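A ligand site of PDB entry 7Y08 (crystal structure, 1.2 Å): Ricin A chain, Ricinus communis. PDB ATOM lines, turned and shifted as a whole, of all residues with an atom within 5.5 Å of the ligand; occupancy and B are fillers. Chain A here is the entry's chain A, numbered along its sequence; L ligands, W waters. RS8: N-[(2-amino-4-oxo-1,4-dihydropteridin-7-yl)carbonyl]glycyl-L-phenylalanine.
O of Gly 128 is in hydrogen-bond range of N1 of the ligand, at 3.2 Å.
An oxygen (O1) of the ligand is in hydrogen-bond range of the guanidinium group of Arg 187 (2.8 Å).
An oxygen (O2) of the ligand is in hydrogen-bond range of the backbone NH (N) of Tyr 130 (2.8 Å).
N of Val 88 lies within hydrogen-bond range of N2 of the ligand (3.0 Å).
A nitrogen (N1) of the ligand lies within hydrogen-bond range of the backbone carbonyl oxygen (O) of Val 88.
A nitrogen (N3) of the ligand lies close to the side-chain hydroxyl (OH) of Tyr 87 (3.4 Å).
An oxygen (O1) of the ligand lies close to the side-chain hydroxyl (OG) of Ser 183 (3.5 Å).
The guanidinium group of Arg 187 lies within salt-bridge range of the side-chain carboxylate of Glu 184 (3.1 Å).
The guanidinium group of Arg 187 is in hydrogen-bond range of the backbone carbonyl oxygen of Asn 85, 2.8 Å away.
The side-chain carboxylate of Glu 184 sits at hydrogen-bond distance from the side-chain hydroxyl of Tyr 130 (2.6 Å).
The backbone NH (N) of Tyr 87 lies close to the side-chain amide oxygen (OD1) of Asn 85 (3.1 Å).
The guanidinium group (NH1) of Arg 141 lies within hydrogen-bond range of the side-chain amide oxygen (OD1) of Asn 216 (2.8 Å).
O of Ile 179 sits at hydrogen-bond distance from N of Glu 184, at 3.0 Å.
OG of Ser 183 is in hydrogen-bond range of O of Ala 86, 2.7 Å away.
The backbone carbonyl oxygen (O) of Val 89 sits at hydrogen-bond distance from the backbone NH (N) of Phe 100, at 3.0 Å.
O of Asn 216 lies close to O3 of the ligand, 3.3 Å away.
Ala 86 touches the ligand (O to O1, 3.5 Å).
Phe 100 touches the ligand (CE2 to N1, 3.5 Å).
Asn 129 touches the ligand (CB to O2, 3.6 Å).
Ile 179 touches the ligand (CG2 to C2, 3.4 Å).
Glu 184 touches the ligand (OE2 to C6, 3.8 Å).
Trp 218 touches the ligand.
N of Gly 219 touches C11 of the ligand, at 3.6 Å.
Hydrophobic or aromatic side chains that line the ligand: Tyr 87, Val 88, Phe 100, Tyr 130, Ile 179 and Trp 218.
Water W6 lies within hydrogen-bond range of the backbone carbonyl oxygen of Glu 215, the side-chain carboxylate of Glu 184 and a nitrogen (N6) of the ligand.
Water W5 lies within hydrogen-bond range of an oxygen (O2) of the ligand, the backbone NH (N) of Asp 131 and the backbone NH (N) of Tyr 130.
Water W4 lies within hydrogen-bond range of an oxygen (O3) of the ligand (2.9 Å) and the backbone carbonyl oxygen of Asn 216 (3.1 Å).
Water W2 bridges an oxygen (O3) of the ligand (3.0 Å) and the side-chain amide oxygen (OD1) of Asn 216 (3.4 Å).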
ATOM      1  N   ASN A  85      23.897  -7.572 -14.814  1.00  0.00           N
ATOM      2  CA  ASN A  85      22.794  -8.125 -15.606  1.00  0.00           C
ATOM      3  C   ASN A  85      22.072  -7.085 -16.490  1.00  0.00           C
ATOM      4  O   ASN A  85      21.087  -7.435 -17.143  1.00  0.00           O
ATOM      5  CB  ASN A  85      21.799  -8.850 -14.689  1.00  0.00           C
ATOM      6  CG  ASN A  85      21.333  -7.998 -13.536  1.00  0.00           C
ATOM      7  OD1 ASN A  85      21.575  -6.785 -13.500  1.00  0.00           O
ATOM      8  ND2 ASN A  85      20.666  -8.609 -12.576  1.00  0.00           N
ATOM      9  N   ALA A  86      22.569  -5.852 -16.498  1.00  0.00           N
ATOM     10  CA  ALA A  86      21.923  -4.696 -17.177  1.00  0.00           C
ATOM     11  C   ALA A  86      20.526  -4.346 -16.649  1.00  0.00           C
ATOM     12  O   ALA A  86      19.779  -3.596 -17.283  1.00  0.00           O
ATOM     13  CB  ALA A  86      21.936  -4.868 -18.703  1.00  0.00           C
ATOM     14  N   TYR A  87      20.190  -4.856 -15.468  1.00  0.00           N
ATOM     15  CA  TYR A  87      18.875  -4.699 -14.866  1.00  0.00           C
ATOM     16  C   TYR A  87      18.646  -3.278 -14.378  1.00  0.00           C
ATOM     17  O   TYR A  87      19.539  -2.679 -13.768  1.00  0.00           O
ATOM     18  CB  TYR A  87      18.760  -5.674 -13.695  1.00  0.00           C
ATOM     19  CG  TYR A  87      17.381  -6.019 -13.218  1.00  0.00           C
ATOM     20  CD1 TYR A  87      16.765  -5.240 -12.235  1.00  0.00           C
ATOM     21  CD2 TYR A  87      16.708  -7.143 -13.702  1.00  0.00           C
ATOM     22  CE1 TYR A  87      15.492  -5.565 -11.770  1.00  0.00           C
ATOM     23  CE2 TYR A  87      15.456  -7.474 -13.239  1.00  0.00           C
ATOM     24  CZ  TYR A  87      14.855  -6.685 -12.273  1.00  0.00           C
ATOM     25  OH  TYR A  87      13.602  -6.998 -11.813  1.00  0.00           O
ATOM     26  N   VAL A  88      17.467  -2.734 -14.671  1.00  0.00           N
ATOM     27  CA  VAL A  88      17.071  -1.419 -14.153  1.00  0.00           C
ATOM     28  C   VAL A  88      16.627  -1.639 -12.703  1.00  0.00           C
ATOM     29  O   VAL A  88      15.587  -2.250 -12.446  1.00  0.00           O
ATOM     30  CB  VAL A  88      15.943  -0.771 -14.997  1.00  0.00           C
ATOM     31  CG1 VAL A  88      15.544   0.581 -14.400  1.00  0.00           C
ATOM     32  CG2 VAL A  88      16.382  -0.608 -16.445  1.00  0.00           C
ATOM     33  N   VAL A  89      17.430  -1.151 -11.765  1.00  0.00           N
ATOM     34  CA  VAL A  89      17.150  -1.379 -10.331  1.00  0.00           C
ATOM     35  C   VAL A  89      16.325  -0.257  -9.694  1.00  0.00           C
ATOM     36  O   VAL A  89      15.768  -0.435  -8.601  1.00  0.00           O
ATOM     37  CB  VAL A  89      18.435  -1.647  -9.511  1.00  0.00           C
ATOM     38  CG1 VAL A  89      19.154  -2.892 -10.011  1.00  0.00           C
ATOM     39  CG2 VAL A  89      19.377  -0.449  -9.492  1.00  0.00           C
ATOM     40  N   PHE A 100      13.155  -0.806  -7.108  1.00  0.00           N
ATOM     41  CA  PHE A 100      12.403  -2.053  -7.040  1.00  0.00           C
ATOM     42  C   PHE A 100      12.812  -2.866  -5.809  1.00  0.00           C
ATOM     43  O   PHE A 100      13.928  -2.724  -5.309  1.00  0.00           O
ATOM     44  CB  PHE A 100      12.588  -2.881  -8.317  1.00  0.00           C
ATOM     45  CG  PHE A 100      12.099  -2.194  -9.562  1.00  0.00           C
ATOM     46  CD1 PHE A 100      10.741  -1.881  -9.723  1.00  0.00           C
ATOM     47  CD2 PHE A 100      12.988  -1.835 -10.574  1.00  0.00           C
ATOM     48  CE1 PHE A 100      10.286  -1.241 -10.868  1.00  0.00           C
ATOM     49  CE2 PHE A 100      12.541  -1.196 -11.731  1.00  0.00           C
ATOM     50  CZ  PHE A 100      11.190  -0.899 -11.878  1.00  0.00           C
ATOM     51  N   GLY A 128      10.911  -5.800  -9.851  1.00  0.00           N
ATOM     52  CA  GLY A 128      10.906  -5.150 -11.161  1.00  0.00           C
ATOM     53  C   GLY A 128      10.851  -6.043 -12.373  1.00  0.00           C
ATOM     54  O   GLY A 128      11.009  -5.555 -13.487  1.00  0.00           O
ATOM     55  N   ASN A 129      10.643  -7.347 -12.174  1.00  0.00           N
ATOM     56  CA  ASN A 129      10.545  -8.295 -13.291  1.00  0.00           C
ATOM     57  C   ASN A 129       9.297  -8.064 -14.143  1.00  0.00           C
ATOM     58  O   ASN A 129       8.305  -7.513 -13.648  1.00  0.00           O
ATOM     59  CB  ASN A 129      10.568  -9.742 -12.781  1.00  0.00           C
ATOM     60  CG  ASN A 129      11.912 -10.147 -12.188  1.00  0.00           C
ATOM     61  OD1 ASN A 129      12.935  -9.490 -12.385  1.00  0.00           O
ATOM     62  ND2 ASN A 129      11.904 -11.260 -11.465  1.00  0.00           N
ATOM     63  N   TYR A 130       9.355  -8.482 -15.405  1.00  0.00           N
ATOM     64  CA  TYR A 130       8.231  -8.289 -16.336  1.00  0.00           C
ATOM     65  C   TYR A 130       6.907  -8.838 -15.826  1.00  0.00           C
ATOM     66  O   TYR A 130       5.896  -8.160 -15.927  1.00  0.00           O
ATOM     67  CB  TYR A 130       8.511  -8.913 -17.704  1.00  0.00           C
ATOM     68  CG  TYR A 130       9.569  -8.224 -18.539  1.00  0.00           C
ATOM     69  CD1 TYR A 130       9.644  -6.826 -18.627  1.00  0.00           C
ATOM     70  CD2 TYR A 130      10.468  -8.976 -19.275  1.00  0.00           C
ATOM     71  CE1 TYR A 130      10.618  -6.204 -19.408  1.00  0.00           C
ATOM     72  CE2 TYR A 130      11.449  -8.383 -20.049  1.00  0.00           C
ATOM     73  CZ  TYR A 130      11.518  -7.006 -20.115  1.00  0.00           C
ATOM     74  OH  TYR A 130      12.486  -6.430 -20.888  1.00  0.00           O
ATOM     75  N   ASP A 131       6.928 -10.052 -15.252  1.00  0.00           N
ATOM     76  CA  ASP A 131       5.727 -10.701 -14.741  1.00  0.00           C
ATOM     77  C   ASP A 131       4.967  -9.811 -13.764  1.00  0.00           C
ATOM     78  O   ASP A 131       3.761  -9.615 -13.922  1.00  0.00           O
ATOM     79  CB  ASP A 131       6.063 -12.068 -14.103  1.00  0.00           C
ATOM     80  CG  ASP A 131       4.821 -12.870 -13.714  1.00  0.00           C
ATOM     81  OD1 ASP A 131       3.812 -12.841 -14.461  1.00  0.00           O
ATOM     82  OD2 ASP A 131       4.855 -13.538 -12.667  1.00  0.00           O
ATOM     83  N   LEU A 133       5.515  -6.428 -13.352  1.00  0.00           N
ATOM     84  CA  LEU A 133       5.205  -5.160 -14.000  1.00  0.00           C
ATOM     85  C   LEU A 133       4.005  -5.239 -14.948  1.00  0.00           C
ATOM     86  O   LEU A 133       3.204  -4.311 -14.998  1.00  0.00           O
ATOM     87  CB  LEU A 133       6.441  -4.588 -14.716  1.00  0.00           C
ATOM     88  CG  LEU A 133       7.622  -4.120 -13.868  1.00  0.00           C
ATOM     89  CD1 LEU A 133       8.709  -3.601 -14.788  1.00  0.00           C
ATOM     90  CD2 LEU A 133       7.258  -3.050 -12.845  1.00  0.00           C
ATOM     91  N   ARG A 141       3.630  -7.482 -22.273  1.00  0.00           N
ATOM     92  CA  ARG A 141       4.594  -6.888 -23.208  1.00  0.00           C
ATOM     93  C   ARG A 141       4.105  -6.900 -24.656  1.00  0.00           C
ATOM     94  O   ARG A 141       4.272  -5.914 -25.371  1.00  0.00           O
ATOM     95  CB  ARG A 141       5.946  -7.591 -23.120  1.00  0.00           C
ATOM     96  CG  ARG A 141       6.838  -7.138 -21.983  1.00  0.00           C
ATOM     97  CD  ARG A 141       8.021  -8.080 -21.848  1.00  0.00           C
ATOM     98  NE  ARG A 141       7.652  -9.351 -21.193  1.00  0.00           N
ATOM     99  CZ  ARG A 141       8.316 -10.496 -21.302  1.00  0.00           C
ATOM    100  NH1 ARG A 141       9.412 -10.582 -22.060  1.00  0.00           N
ATOM    101  NH2 ARG A 141       7.897 -11.559 -20.644  1.00  0.00           N
ATOM    102  N   ILE A 179      12.824  -0.503 -19.981  1.00  0.00           N
ATOM    103  CA  ILE A 179      13.612  -1.719 -19.842  1.00  0.00           C
ATOM    104  C   ILE A 179      13.926  -2.331 -21.214  1.00  0.00           C
ATOM    105  O   ILE A 179      15.063  -2.688 -21.494  1.00  0.00           O
ATOM    106  CB  ILE A 179      12.924  -2.746 -18.911  1.00  0.00           C
ATOM    107  CG1 ILE A 179      12.901  -2.222 -17.461  1.00  0.00           C
ATOM    108  CG2 ILE A 179      13.636  -4.091 -18.950  1.00  0.00           C
ATOM    109  CD1 ILE A 179      11.775  -2.779 -16.620  1.00  0.00           C
ATOM    110  N   SER A 183      17.796  -1.760 -21.667  1.00  0.00           N
ATOM    111  CA  SER A 183      18.436  -3.001 -21.209  1.00  0.00           C
ATOM    112  C   SER A 183      18.391  -4.114 -22.247  1.00  0.00           C
ATOM    113  O   SER A 183      19.417  -4.720 -22.543  1.00  0.00           O
ATOM    114  CB  SER A 183      17.833  -3.470 -19.879  1.00  0.00           C
ATOM    115  OG  SER A 183      17.953  -2.448 -18.904  1.00  0.00           O
ATOM    116  N   GLU A 184      17.211  -4.381 -22.819  1.00  0.00           N
ATOM    117  CA  GLU A 184      17.093  -5.467 -23.796  1.00  0.00           C
ATOM    118  C   GLU A 184      17.828  -5.158 -25.091  1.00  0.00           C
ATOM    119  O   GLU A 184      18.437  -6.028 -25.687  1.00  0.00           O
ATOM    120  CB  GLU A 184      15.633  -5.832 -24.091  1.00  0.00           C
ATOM    121  CG  GLU A 184      14.820  -6.278 -22.875  1.00  0.00           C
ATOM    122  CD  GLU A 184      15.206  -7.624 -22.283  1.00  0.00           C
ATOM    123  OE1 GLU A 184      16.253  -8.211 -22.625  1.00  0.00           O
ATOM    124  OE2 GLU A 184      14.430  -8.093 -21.425  1.00  0.00           O
ATOM    125  N   ARG A 187      21.402  -5.828 -24.421  1.00  0.00           N
ATOM    126  CA  ARG A 187      21.634  -7.274 -24.382  1.00  0.00           C
ATOM    127  C   ARG A 187      21.624  -7.926 -25.767  1.00  0.00           C
ATOM    128  O   ARG A 187      22.370  -8.883 -25.999  1.00  0.00           O
ATOM    129  CB  ARG A 187      20.589  -7.964 -23.514  1.00  0.00           C
ATOM    130  CG  ARG A 187      20.694  -7.693 -22.023  1.00  0.00           C
ATOM    131  CD  ARG A 187      19.448  -8.186 -21.319  1.00  0.00           C
ATOM    132  NE  ARG A 187      19.437  -7.788 -19.918  1.00  0.00           N
ATOM    133  CZ  ARG A 187      18.361  -7.390 -19.247  1.00  0.00           C
ATOM    134  NH1 ARG A 187      17.170  -7.335 -19.842  1.00  0.00           N
ATOM    135  NH2 ARG A 187      18.461  -7.041 -17.965  1.00  0.00           N
ATOM    136  N   GLU A 215      13.948 -12.020 -25.107  1.00  0.00           N
ATOM    137  CA  GLU A 215      13.911 -11.442 -23.752  1.00  0.00           C
ATOM    138  C   GLU A 215      13.781 -12.526 -22.691  1.00  0.00           C
ATOM    139  O   GLU A 215      14.575 -12.590 -21.756  1.00  0.00           O
ATOM    140  CB  GLU A 215      12.763 -10.443 -23.613  1.00  0.00           C
ATOM    141  CG  GLU A 215      12.932  -9.197 -24.456  1.00  0.00           C
ATOM    142  CD  GLU A 215      11.732  -8.273 -24.418  1.00  0.00           C
ATOM    143  OE1 GLU A 215      10.696  -8.623 -23.804  1.00  0.00           O
ATOM    144  OE2 GLU A 215      11.823  -7.192 -25.021  1.00  0.00           O
ATOM    145  N   ASN A 216      12.789 -13.400 -22.882  1.00  0.00           N
ATOM    146  CA  ASN A 216      12.527 -14.482 -21.935  1.00  0.00           C
ATOM    147  C   ASN A 216      13.642 -15.506 -21.835  1.00  0.00           C
ATOM    148  O   ASN A 216      13.796 -16.154 -20.799  1.00  0.00           O
ATOM    149  CB  ASN A 216      11.207 -15.168 -22.285  1.00  0.00           C
ATOM    150  CG  ASN A 216       9.990 -14.285 -22.063  1.00  0.00           C
ATOM    151  OD1 ASN A 216      10.067 -13.257 -21.373  1.00  0.00           O
ATOM    152  ND2 ASN A 216       8.870 -14.678 -22.637  1.00  0.00           N
ATOM    153  N   SER A 217      14.422 -15.643 -22.900  1.00  0.00           N
ATOM    154  CA  SER A 217      15.464 -16.665 -22.995  1.00  0.00           C
ATOM    155  C   SER A 217      16.884 -16.179 -22.701  1.00  0.00           C
ATOM    156  O   SER A 217      17.818 -16.960 -22.797  1.00  0.00           O
ATOM    157  CB  SER A 217      15.440 -17.322 -24.372  1.00  0.00           C
ATOM    158  OG  SER A 217      14.163 -17.877 -24.648  1.00  0.00           O
ATOM    159  N   TRP A 218      17.052 -14.897 -22.349  1.00  0.00           N
ATOM    160  CA  TRP A 218      18.388 -14.328 -22.179  1.00  0.00           C
ATOM    161  C   TRP A 218      19.254 -15.097 -21.187  1.00  0.00           C
ATOM    162  O   TRP A 218      20.417 -15.385 -21.473  1.00  0.00           O
ATOM    163  CB  TRP A 218      18.335 -12.849 -21.762  1.00  0.00           C
ATOM    164  CG  TRP A 218      19.692 -12.194 -21.728  1.00  0.00           C
ATOM    165  CD1 TRP A 218      20.583 -12.093 -22.760  1.00  0.00           C
ATOM    166  CD2 TRP A 218      20.309 -11.548 -20.609  1.00  0.00           C
ATOM    167  NE1 TRP A 218      21.705 -11.415 -22.357  1.00  0.00           N
ATOM    168  CE2 TRP A 218      21.570 -11.070 -21.044  1.00  0.00           C
ATOM    169  CE3 TRP A 218      19.917 -11.315 -19.280  1.00  0.00           C
ATOM    170  CZ2 TRP A 218      22.447 -10.373 -20.194  1.00  0.00           C
ATOM    171  CZ3 TRP A 218      20.786 -10.624 -18.433  1.00  0.00           C
ATOM    172  CH2 TRP A 218      22.034 -10.156 -18.909  1.00  0.00           C
ATOM    173  N   GLY A 219      18.679 -15.432 -20.033  1.00  0.00           N
ATOM    174  CA  GLY A 219      19.388 -16.197 -19.005  1.00  0.00           C
ATOM    175  C   GLY A 219      19.786 -17.579 -19.492  1.00  0.00           C
ATOM    176  O   GLY A 219      20.928 -18.001 -19.314  1.00  0.00           O
ATOM    177  N   VAL A 263      24.876 -12.535 -19.287  1.00  0.00           N
ATOM    178  CA  VAL A 263      25.063 -12.567 -17.831  1.00  0.00           C
ATOM    179  C   VAL A 263      26.097 -13.651 -17.501  1.00  0.00           C
ATOM    180  O   VAL A 263      26.098 -14.727 -18.115  1.00  0.00           O
ATOM    181  CB  VAL A 263      23.707 -12.755 -17.069  1.00  0.00           C
ATOM    182  CG1 VAL A 263      22.966 -14.015 -17.492  1.00  0.00           C
ATOM    183  CG2 VAL A 263      23.904 -12.722 -15.553  1.00  0.00           C
ATOM    184  N   ARG A 265      27.757 -16.674 -15.777  1.00  0.00           N
ATOM    185  CA  ARG A 265      27.288 -17.889 -15.113  1.00  0.00           C
ATOM    186  C   ARG A 265      28.410 -18.685 -14.469  1.00  0.00           C
ATOM    187  O   ARG A 265      28.217 -19.322 -13.440  1.00  0.00           O
ATOM    188  CB  ARG A 265      26.498 -18.764 -16.088  1.00  0.00           C
ATOM    189  CG  ARG A 265      25.186 -18.167 -16.558  1.00  0.00           C
ATOM    190  CD  ARG A 265      24.175 -18.112 -15.437  1.00  0.00           C
ATOM    191  NE  ARG A 265      22.813 -17.906 -15.925  1.00  0.00           N
ATOM    192  CZ  ARG A 265      21.999 -16.924 -15.529  1.00  0.00           C
ATOM    193  NH1 ARG A 265      22.380 -16.033 -14.616  1.00  0.00           N
ATOM    194  NH2 ARG A 265      20.784 -16.844 -16.041  1.00  0.00           N
HETATM  195  C1  RS8 L   1      14.032  -4.634 -14.837  1.00  0.00           C
HETATM  196  N1  RS8 L   1      13.633  -3.728 -13.931  1.00  0.00           N
HETATM  197  O1  RS8 L   1      16.594  -5.131 -17.182  1.00  0.00           O
HETATM  198  C2  RS8 L   1      15.560  -5.347 -16.504  1.00  0.00           C
HETATM  199  N2  RS8 L   1      15.154  -4.440 -15.585  1.00  0.00           N
HETATM  200  C3  RS8 L   1      14.818  -6.516 -16.702  1.00  0.00           C
HETATM  201  N3  RS8 L   1      13.273  -5.747 -14.992  1.00  0.00           N
HETATM  202  O2  RS8 L   1      11.469 -10.149 -16.221  1.00  0.00           O
HETATM  203  C4  RS8 L   1      13.602  -6.705 -15.871  1.00  0.00           C
HETATM  204  N4  RS8 L   1      12.864  -7.820 -16.004  1.00  0.00           N
HETATM  205  C5  RS8 L   1      13.228  -8.756 -16.904  1.00  0.00           C
HETATM  206  N5  RS8 L   1      15.148  -7.481 -17.596  1.00  0.00           N
HETATM  207  C6  RS8 L   1      14.373  -8.577 -17.695  1.00  0.00           C
HETATM  208  C7  RS8 L   1      12.381 -10.001 -17.019  1.00  0.00           C
HETATM  209  N6  RS8 L   1      12.660 -10.913 -17.941  1.00  0.00           N
HETATM  210  C8  RS8 L   1      11.958 -12.162 -18.208  1.00  0.00           C
HETATM  211  C9  RS8 L   1      12.822 -13.369 -18.006  1.00  0.00           C
HETATM  212  O3  RS8 L   1      12.386 -14.461 -18.355  1.00  0.00           O
HETATM  213  N7  RS8 L   1      14.027 -13.183 -17.446  1.00  0.00           N
HETATM  214  C10 RS8 L   1      14.977 -14.258 -17.169  1.00  0.00           C
HETATM  215  C18 RS8 L   1      15.115 -14.545 -15.697  1.00  0.00           C
HETATM  216  O5  RS8 L   1      15.749 -15.552 -15.336  1.00  0.00           O
HETATM  217  C11 RS8 L   1      16.303 -13.853 -17.842  1.00  0.00           C
HETATM  218  C12 RS8 L   1      16.990 -12.660 -17.204  1.00  0.00           C
HETATM  219  C13 RS8 L   1      17.929 -12.862 -16.187  1.00  0.00           C
HETATM  220  C17 RS8 L   1      16.688 -11.359 -17.626  1.00  0.00           C
HETATM  221  C14 RS8 L   1      18.572 -11.773 -15.587  1.00  0.00           C
HETATM  222  C16 RS8 L   1      17.323 -10.264 -17.022  1.00  0.00           C
HETATM  223  C15 RS8 L   1      18.261 -10.471 -15.996  1.00  0.00           C
HETATM  224  O4  RS8 L   1      14.588 -13.755 -14.869  1.00  0.00           O
HETATM  225  O   HOH W   1      20.322 -14.211 -14.011  1.00  0.00           O
HETATM  226  O   HOH W   2       9.394 -14.693 -18.396  1.00  0.00           O
HETATM  227  O   HOH W   3      16.676 -11.131 -12.926  1.00  0.00           O
HETATM  228  O   HOH W   4      12.295 -17.409 -18.379  1.00  0.00           O
HETATM  229  O   HOH W   5       9.276 -11.955 -15.464  1.00  0.00           O
HETATM  230  O   HOH W   6      14.459 -10.457 -20.149  1.00  0.00           O
